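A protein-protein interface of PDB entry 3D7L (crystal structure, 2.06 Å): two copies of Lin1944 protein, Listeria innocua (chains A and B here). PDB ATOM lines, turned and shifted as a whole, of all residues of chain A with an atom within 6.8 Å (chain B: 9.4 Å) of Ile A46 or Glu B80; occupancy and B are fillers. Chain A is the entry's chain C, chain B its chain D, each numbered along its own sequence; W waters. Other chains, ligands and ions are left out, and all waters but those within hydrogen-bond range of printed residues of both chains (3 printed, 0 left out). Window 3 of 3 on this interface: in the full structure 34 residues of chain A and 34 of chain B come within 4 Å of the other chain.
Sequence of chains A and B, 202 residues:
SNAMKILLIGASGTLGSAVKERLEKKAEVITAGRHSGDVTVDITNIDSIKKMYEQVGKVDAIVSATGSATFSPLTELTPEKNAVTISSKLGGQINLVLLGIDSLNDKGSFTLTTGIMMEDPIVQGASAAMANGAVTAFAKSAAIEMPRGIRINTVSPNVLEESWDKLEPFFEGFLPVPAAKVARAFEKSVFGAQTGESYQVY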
ATOM      1  N   ASP A  42     -27.623  29.157  31.033  1.00  0.00           N
ATOM      2  CA  ASP A  42     -28.658  28.438  30.350  1.00  0.00           C
ATOM      3  C   ASP A  42     -28.169  26.994  30.290  1.00  0.00           C
ATOM      4  O   ASP A  42     -27.274  26.661  29.524  1.00  0.00           O
ATOM      5  CB  ASP A  42     -28.863  29.052  28.959  1.00  0.00           C
ATOM      6  CG  ASP A  42     -29.859  28.298  28.121  1.00  0.00           C
ATOM      7  OD1 ASP A  42     -30.302  27.198  28.498  1.00  0.00           O
ATOM      8  OD2 ASP A  42     -30.204  28.820  27.045  1.00  0.00           O
ATOM      9  N   ILE A  43     -28.740  26.143  31.127  1.00  0.00           N
ATOM     10  CA  ILE A  43     -28.318  24.757  31.193  1.00  0.00           C
ATOM     11  C   ILE A  43     -28.586  23.942  29.917  1.00  0.00           C
ATOM     12  O   ILE A  43     -28.057  22.839  29.785  1.00  0.00           O
ATOM     13  CB  ILE A  43     -28.871  24.020  32.433  1.00  0.00           C
ATOM     14  CG1 ILE A  43     -30.373  23.756  32.296  1.00  0.00           C
ATOM     15  CG2 ILE A  43     -28.496  24.788  33.676  1.00  0.00           C
ATOM     16  CD1 ILE A  43     -30.915  22.690  33.223  1.00  0.00           C
ATOM     17  N   THR A  44     -29.370  24.477  28.984  1.00  0.00           N
ATOM     18  CA  THR A  44     -29.491  23.812  27.675  1.00  0.00           C
ATOM     19  C   THR A  44     -28.362  24.145  26.689  1.00  0.00           C
ATOM     20  O   THR A  44     -28.335  23.586  25.601  1.00  0.00           O
ATOM     21  CB  THR A  44     -30.851  24.068  26.970  1.00  0.00           C
ATOM     22  OG1 THR A  44     -30.864  25.391  26.450  1.00  0.00           O
ATOM     23  CG2 THR A  44     -32.005  23.877  27.925  1.00  0.00           C
ATOM     24  N   ASN A  45     -27.437  25.035  27.061  1.00  0.00           N
ATOM     25  CA  ASN A  45     -26.327  25.453  26.190  1.00  0.00           C
ATOM     26  C   ASN A  45     -24.962  25.118  26.815  1.00  0.00           C
ATOM     27  O   ASN A  45     -24.585  25.696  27.843  1.00  0.00           O
ATOM     28  CB  ASN A  45     -26.434  26.969  25.909  1.00  0.00           C
ATOM     29  CG  ASN A  45     -25.494  27.449  24.783  1.00  0.00           C
ATOM     30  OD1 ASN A  45     -24.416  26.904  24.552  1.00  0.00           O
ATOM     31  ND2 ASN A  45     -25.912  28.480  24.098  1.00  0.00           N
ATOM     32  N   ILE A  46     -24.204  24.195  26.214  1.00  0.00           N
ATOM     33  CA  ILE A  46     -22.947  23.796  26.871  1.00  0.00           C
ATOM     34  C   ILE A  46     -21.952  24.957  26.946  1.00  0.00           C
ATOM     35  O   ILE A  46     -21.172  25.037  27.896  1.00  0.00           O
ATOM     36  CB  ILE A  46     -22.288  22.473  26.336  1.00  0.00           C
ATOM     37  CG1 ILE A  46     -21.528  22.697  25.028  1.00  0.00           C
ATOM     38  CG2 ILE A  46     -23.321  21.359  26.264  1.00  0.00           C
ATOM     39  CD1 ILE A  46     -20.877  21.408  24.460  1.00  0.00           C
ATOM     40  N   ASP A  47     -21.993  25.860  25.961  1.00  0.00           N
ATOM     41  CA  ASP A  47     -21.109  27.036  26.005  1.00  0.00           C
ATOM     42  C   ASP A  47     -21.399  27.956  27.191  1.00  0.00           C
ATOM     43  O   ASP A  47     -20.476  28.489  27.803  1.00  0.00           O
ATOM     44  CB  ASP A  47     -21.116  27.782  24.671  1.00  0.00           C
ATOM     45  CG  ASP A  47     -20.350  27.023  23.590  1.00  0.00           C
ATOM     46  OD1 ASP A  47     -19.344  26.354  23.953  1.00  0.00           O
ATOM     47  OD2 ASP A  47     -20.753  27.084  22.397  1.00  0.00           O
ATOM     48  N   SER A  48     -22.679  28.103  27.521  1.00  0.00           N
ATOM     49  CA  SER A  48     -23.142  28.797  28.727  1.00  0.00           C
ATOM     50  C   SER A  48     -22.660  28.132  30.039  1.00  0.00           C
ATOM     51  O   SER A  48     -22.104  28.797  30.910  1.00  0.00           O
ATOM     52  CB  SER A  48     -24.666  28.893  28.710  1.00  0.00           C
ATOM     53  OG  SER A  48     -25.146  29.644  29.803  1.00  0.00           O
ATOM     54  N   ILE A  49     -22.879  26.826  30.176  1.00  0.00           N
ATOM     55  CA  ILE A  49     -22.365  26.082  31.340  1.00  0.00           C
ATOM     56  C   ILE A  49     -20.840  26.265  31.474  1.00  0.00           C
ATOM     57  O   ILE A  49     -20.303  26.459  32.575  1.00  0.00           O
ATOM     58  CB  ILE A  49     -22.715  24.551  31.246  1.00  0.00           C
ATOM     59  CG1 ILE A  49     -24.239  24.321  31.171  1.00  0.00           C
ATOM     60  CG2 ILE A  49     -22.068  23.783  32.376  1.00  0.00           C
ATOM     61  CD1 ILE A  49     -24.663  22.903  30.701  1.00  0.00           C
ATOM     62  N   LYS A  50     -20.131  26.175  30.360  1.00  0.00           N
ATOM     63  CA  LYS A  50     -18.677  26.253  30.421  1.00  0.00           C
ATOM     64  C   LYS A  50     -18.238  27.628  30.942  1.00  0.00           C
ATOM     65  O   LYS A  50     -17.298  27.726  31.719  1.00  0.00           O
ATOM     66  CB  LYS A  50     -18.053  25.996  29.059  1.00  0.00           C
ATOM     67  CG  LYS A  50     -17.964  24.557  28.610  1.00  0.00           C
ATOM     68  CD  LYS A  50     -17.146  24.527  27.326  1.00  0.00           C
ATOM     69  CE  LYS A  50     -16.911  23.111  26.828  1.00  0.00           C
ATOM     70  NZ  LYS A  50     -17.948  22.687  25.857  1.00  0.00           N
ATOM     71  N   LYS A  51     -18.948  28.673  30.527  1.00  0.00           N
ATOM     72  CA  LYS A  51     -18.585  30.028  30.918  1.00  0.00           C
ATOM     73  C   LYS A  51     -18.960  30.286  32.368  1.00  0.00           C
ATOM     74  O   LYS A  51     -18.229  30.974  33.056  1.00  0.00           O
ATOM     75  CB  LYS A  51     -19.153  31.089  29.969  1.00  0.00           C
ATOM     76  CG  LYS A  51     -18.229  32.279  29.873  1.00  0.00           C
ATOM     77  CD  LYS A  51     -18.866  33.515  29.267  1.00  0.00           C
ATOM     78  CE  LYS A  51     -17.853  34.694  29.292  1.00  0.00           C
ATOM     79  NZ  LYS A  51     -18.270  35.872  28.431  1.00  0.00           N
ATOM     80  N   ASN A  95     -25.133  17.539  32.133  1.00  0.00           N
ATOM     81  CA  ASN A  95     -24.043  18.354  31.627  1.00  0.00           C
ATOM     82  C   ASN A  95     -23.334  19.215  32.627  1.00  0.00           C
ATOM     83  O   ASN A  95     -22.150  19.499  32.467  1.00  0.00           O
ATOM     84  CB  ASN A  95     -24.475  19.186  30.401  1.00  0.00           C
ATOM     85  CG  ASN A  95     -24.508  18.341  29.154  1.00  0.00           C
ATOM     86  OD1 ASN A  95     -24.097  17.174  29.206  1.00  0.00           O
ATOM     87  ND2 ASN A  95     -25.030  18.885  28.041  1.00  0.00           N
ATOM     88  N   LEU A  98     -20.902  16.629  33.852  1.00  0.00           N
ATOM     89  CA  LEU A  98     -19.869  16.363  32.847  1.00  0.00           C
ATOM     90  C   LEU A  98     -18.917  17.544  32.681  1.00  0.00           C
ATOM     91  O   LEU A  98     -17.725  17.346  32.462  1.00  0.00           O
ATOM     92  CB  LEU A  98     -20.471  15.937  31.500  1.00  0.00           C
ATOM     93  CG  LEU A  98     -21.422  14.720  31.494  1.00  0.00           C
ATOM     94  CD1 LEU A  98     -21.901  14.375  30.084  1.00  0.00           C
ATOM     95  CD2 LEU A  98     -20.771  13.489  32.118  1.00  0.00           C
ATOM     96  N   LEU A  99     -19.415  18.768  32.831  1.00  0.00           N
ATOM     97  CA  LEU A  99     -18.553  19.939  32.636  1.00  0.00           C
ATOM     98  C   LEU A  99     -18.040  20.583  33.941  1.00  0.00           C
ATOM     99  O   LEU A  99     -17.240  21.516  33.887  1.00  0.00           O
ATOM    100  CB  LEU A  99     -19.240  20.974  31.727  1.00  0.00           C
ATOM    101  CG  LEU A  99     -19.596  20.491  30.302  1.00  0.00           C
ATOM    102  CD1 LEU A  99     -20.782  21.306  29.759  1.00  0.00           C
ATOM    103  CD2 LEU A  99     -18.369  20.571  29.330  1.00  0.00           C
ATOM    104  N   THR B  70     -22.830   5.258  24.553  1.00  0.00           N
ATOM    105  CA  THR B  70     -21.398   5.507  24.721  1.00  0.00           C
ATOM    106  C   THR B  70     -20.871   4.790  25.962  1.00  0.00           C
ATOM    107  O   THR B  70     -21.474   4.897  27.047  1.00  0.00           O
ATOM    108  CB  THR B  70     -21.100   7.020  24.825  1.00  0.00           C
ATOM    109  OG1 THR B  70     -21.318   7.610  23.544  1.00  0.00           O
ATOM    110  CG2 THR B  70     -19.663   7.276  25.231  1.00  0.00           C
ATOM    111  N   SER B  72     -17.702   5.086  27.736  1.00  0.00           N
ATOM    112  CA  SER B  72     -16.502   5.901  28.007  1.00  0.00           C
ATOM    113  C   SER B  72     -16.281   6.064  29.532  1.00  0.00           C
ATOM    114  O   SER B  72     -17.252   6.145  30.292  1.00  0.00           O
ATOM    115  CB  SER B  72     -16.702   7.290  27.375  1.00  0.00           C
ATOM    116  OG  SER B  72     -15.821   8.267  27.932  1.00  0.00           O
ATOM    117  N   GLU B  76     -13.838  11.160  30.746  1.00  0.00           N
ATOM    118  CA  GLU B  76     -13.688  11.298  29.285  1.00  0.00           C
ATOM    119  C   GLU B  76     -15.039  11.469  28.612  1.00  0.00           C
ATOM    120  O   GLU B  76     -15.119  11.593  27.392  1.00  0.00           O
ATOM    121  CB  GLU B  76     -13.038  10.037  28.698  1.00  0.00           C
ATOM    122  CG  GLU B  76     -11.526  10.052  28.580  1.00  0.00           C
ATOM    123  CD  GLU B  76     -10.838  10.609  29.802  1.00  0.00           C
ATOM    124  OE1 GLU B  76     -10.294  11.728  29.689  1.00  0.00           O
ATOM    125  OE2 GLU B  76     -10.853   9.950  30.874  1.00  0.00           O
ATOM    126  N   LEU B  77     -16.101  11.417  29.408  1.00  0.00           N
ATOM    127  CA  LEU B  77     -17.459  11.462  28.887  1.00  0.00           C
ATOM    128  C   LEU B  77     -17.875  12.929  28.706  1.00  0.00           C
ATOM    129  O   LEU B  77     -18.181  13.618  29.666  1.00  0.00           O
ATOM    130  CB  LEU B  77     -18.416  10.732  29.831  1.00  0.00           C
ATOM    131  CG  LEU B  77     -19.906  10.638  29.476  1.00  0.00           C
ATOM    132  CD1 LEU B  77     -20.140  10.108  28.053  1.00  0.00           C
ATOM    133  CD2 LEU B  77     -20.638   9.811  30.529  1.00  0.00           C
ATOM    134  N   THR B  78     -17.850  13.413  27.479  1.00  0.00           N
ATOM    135  CA  THR B  78     -18.233  14.793  27.219  1.00  0.00           C
ATOM    136  C   THR B  78     -19.723  14.886  26.899  1.00  0.00           C
ATOM    137  O   THR B  78     -20.346  13.877  26.587  1.00  0.00           O
ATOM    138  CB  THR B  78     -17.434  15.384  26.038  1.00  0.00           C
ATOM    139  OG1 THR B  78     -17.771  14.681  24.835  1.00  0.00           O
ATOM    140  CG2 THR B  78     -15.944  15.283  26.298  1.00  0.00           C
ATOM    141  N   PRO B  79     -20.288  16.111  26.914  1.00  0.00           N
ATOM    142  CA  PRO B  79     -21.648  16.267  26.391  1.00  0.00           C
ATOM    143  C   PRO B  79     -21.847  15.653  24.983  1.00  0.00           C
ATOM    144  O   PRO B  79     -22.863  14.980  24.753  1.00  0.00           O
ATOM    145  CB  PRO B  79     -21.826  17.786  26.346  1.00  0.00           C
ATOM    146  CG  PRO B  79     -20.930  18.276  27.468  1.00  0.00           C
ATOM    147  CD  PRO B  79     -19.728  17.392  27.381  1.00  0.00           C
ATOM    148  N   GLU B  80     -20.883  15.853  24.080  1.00  0.00           N
ATOM    149  CA  GLU B  80     -20.972  15.332  22.714  1.00  0.00           C
ATOM    150  C   GLU B  80     -21.061  13.818  22.706  1.00  0.00           C
ATOM    151  O   GLU B  80     -21.902  13.257  22.018  1.00  0.00           O
ATOM    152  CB  GLU B  80     -19.775  15.780  21.857  1.00  0.00           C
ATOM    153  CG  GLU B  80     -19.768  17.261  21.494  1.00  0.00           C
ATOM    154  CD  GLU B  80     -19.190  18.167  22.598  1.00  0.00           C
ATOM    155  OE1 GLU B  80     -18.951  17.682  23.733  1.00  0.00           O
ATOM    156  OE2 GLU B  80     -18.973  19.369  22.319  1.00  0.00           O
ATOM    157  N   LYS B  81     -20.213  13.166  23.500  1.00  0.00           N
ATOM    158  CA  LYS B  81     -20.210  11.700  23.607  1.00  0.00           C
ATOM    159  C   LYS B  81     -21.505  11.180  24.193  1.00  0.00           C
ATOM    160  O   LYS B  81     -22.055  10.177  23.747  1.00  0.00           O
ATOM    161  CB  LYS B  81     -19.013  11.203  24.428  1.00  0.00           C
ATOM    162  CG  LYS B  81     -17.732  11.209  23.640  1.00  0.00           C
ATOM    163  CD  LYS B  81     -16.538  10.839  24.481  1.00  0.00           C
ATOM    164  CE  LYS B  81     -15.302  11.388  23.796  1.00  0.00           C
ATOM    165  NZ  LYS B  81     -14.107  11.337  24.658  1.00  0.00           N
ATOM    166  N   ASN B  82     -22.010  11.903  25.179  1.00  0.00           N
ATOM    167  CA  ASN B  82     -23.217  11.506  25.886  1.00  0.00           C
ATOM    168  C   ASN B  82     -24.481  11.688  25.017  1.00  0.00           C
ATOM    169  O   ASN B  82     -25.480  10.972  25.188  1.00  0.00           O
ATOM    170  CB  ASN B  82     -23.297  12.293  27.198  1.00  0.00           C
ATOM    171  CG  ASN B  82     -24.237  11.671  28.205  1.00  0.00           C
ATOM    172  OD1 ASN B  82     -25.118  12.352  28.727  1.00  0.00           O
ATOM    173  ND2 ASN B  82     -24.044  10.396  28.510  1.00  0.00           N
ATOM    174  N   ALA B  83     -24.418  12.646  24.099  1.00  0.00           N
ATOM    175  CA  ALA B  83     -25.468  12.937  23.123  1.00  0.00           C
ATOM    176  C   ALA B  83     -25.760  11.776  22.198  1.00  0.00           C
ATOM    177  O   ALA B  83     -26.883  11.639  21.686  1.00  0.00           O
ATOM    178  CB  ALA B  83     -25.077  14.177  22.287  1.00  0.00           C
ATOM    179  N   VAL B  84     -24.757  10.944  21.972  1.00  0.00           N
ATOM    180  CA  VAL B  84     -24.920   9.746  21.143  1.00  0.00           C
ATOM    181  C   VAL B  84     -25.864   8.755  21.848  1.00  0.00           C
ATOM    182  O   VAL B  84     -26.860   8.306  21.272  1.00  0.00           O
ATOM    183  CB  VAL B  84     -23.530   9.099  20.779  1.00  0.00           C
ATOM    184  CG1 VAL B  84     -23.720   7.905  19.883  1.00  0.00           C
ATOM    185  CG2 VAL B  84     -22.606  10.131  20.098  1.00  0.00           C
ATOM    186  N   THR B  85     -25.574   8.448  23.110  1.00  0.00           N
ATOM    187  CA  THR B  85     -26.493   7.631  23.925  1.00  0.00           C
ATOM    188  C   THR B  85     -27.912   8.204  23.875  1.00  0.00           C
ATOM    189  O   THR B  85     -28.891   7.476  23.623  1.00  0.00           O
ATOM    190  CB  THR B  85     -26.053   7.617  25.376  1.00  0.00           C
ATOM    191  OG1 THR B  85     -24.683   7.253  25.419  1.00  0.00           O
ATOM    192  CG2 THR B  85     -26.900   6.600  26.209  1.00  0.00           C
ATOM    193  N   ILE B  86     -27.999   9.513  24.118  1.00  0.00           N
ATOM    194  CA  ILE B  86     -29.273  10.223  24.154  1.00  0.00           C
ATOM    195  C   ILE B  86     -30.089  10.028  22.885  1.00  0.00           C
ATOM    196  O   ILE B  86     -31.310   9.845  22.973  1.00  0.00           O
ATOM    197  CB  ILE B  86     -29.105  11.714  24.508  1.00  0.00           C
ATOM    198  CG1 ILE B  86     -28.646  11.846  25.977  1.00  0.00           C
ATOM    199  CG2 ILE B  86     -30.416  12.470  24.299  1.00  0.00           C
ATOM    200  CD1 ILE B  86     -28.367  13.267  26.434  1.00  0.00           C
ATOM    201  N   SER B  87     -29.431  10.009  21.722  1.00  0.00           N
ATOM    202  CA  SER B  87     -30.170   9.836  20.462  1.00  0.00           C
ATOM    203  C   SER B  87     -30.524   8.388  20.154  1.00  0.00           C
ATOM    204  O   SER B  87     -31.433   8.140  19.363  1.00  0.00           O
ATOM    205  CB  SER B  87     -29.440  10.486  19.261  1.00  0.00           C
ATOM    206  OG  SER B  87     -28.345   9.681  18.860  1.00  0.00           O
ATOM    207  N   SER B 127     -23.112   6.430  31.088  1.00  0.00           N
ATOM    208  CA  SER B 127     -23.987   6.853  30.021  1.00  0.00           C
ATOM    209  C   SER B 127     -25.020   5.762  29.695  1.00  0.00           C
ATOM    210  O   SER B 127     -26.193   6.051  29.469  1.00  0.00           O
ATOM    211  CB  SER B 127     -23.142   7.230  28.813  1.00  0.00           C
ATOM    212  OG  SER B 127     -23.949   7.729  27.770  1.00  0.00           O
HETATM  213  O   HOH W   1     -16.497  14.338  32.101  1.00  0.00           O
HETATM  214  O   HOH W   2     -17.722  19.481  25.335  1.00  0.00           O
HETATM  215  O   HOH W   3     -25.551  15.140  28.318  1.00  0.00           O
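N of Leu B77 sits at hydrogen-bond distance from OG of Ser B72, 3.5 Å away.
The side-chain carboxylate of Glu B80 lies within hydrogen-bond range of the side-chain hydroxyl of Thr B78, at 3.4 Å.
The backbone NH of Lys B81 sits at hydrogen-bond distance from the side-chain hydroxyl of Thr B78 (3.2 Å).
ND2 of Asn B82 is in hydrogen-bond range of OG of Ser B127 (2.8 Å).
Pro B79 touches Ile A46 (CB to CG2, 3.9 Å).
Ile A46 touches Glu B80 (CD1 to OE2, 3.5 Å).
OD1 of Asn A95 touches CB of Pro B79, 3.7 Å away.
Leu A98 touches Leu B77.
Thr B78 touches Leu A98.
Pro B79 touches Leu A98 (N to CD1, 3.96 Å).
Leu A98 touches Asn B82.
Leu A99 touches Pro B79 (CD1 to CG, 3.8 Å).
Glu B80 touches one residue of chain A.
No residue of chain B comes within 4 Å of Asp A47.
No residue of chain B comes within 4 Å of Ile A49.
Of the printed residues of chain A, Leu B77 touches Leu A98.
Printed residues of chain B within 4 Å of Asn A95: Pro B79 (3.7 Å).
Printed residues of chain A within 4 Å of Pro B79: Ile A46, Asn A95, Leu A98 and Leu A99.
Printed residues of chain B within 4 Å of Leu A98: Leu B77, Thr B78, Pro B79 and Asn B82.
Of the printed residues of chain A, Asn B82 touches Leu A98.
The nearest residue of chain B that does not touch Ile A46 is Thr B78 (7.1 Å).
The nearest residue of chain A that does not touch Glu B80 is Lys A50 (5.0 Å).
The nearest printed residue of chain B that does not touch Leu A98 is Glu B80 (6.3 Å).
Hydrophobic or aromatic side chains of chain B that line the printed part of chain A: Leu B77 and Pro B79.
Among the printed residues, 8 pairs touch across the chains.
No position is printed for both chains.
Water W3 lies within hydrogen-bond range of the side-chain amide oxygen of Asn A95 (2.7 Å) and the side-chain amide oxygen of Asn B82 (2.9 Å).
Water W2 bridges OE1 of Glu B80 (2.7 Å) and NZ of Lys A50 (3.3 Å).
Water W1 bridges O of Leu B77 (3.0 Å) and O of Leu A98 (3.3 Å).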
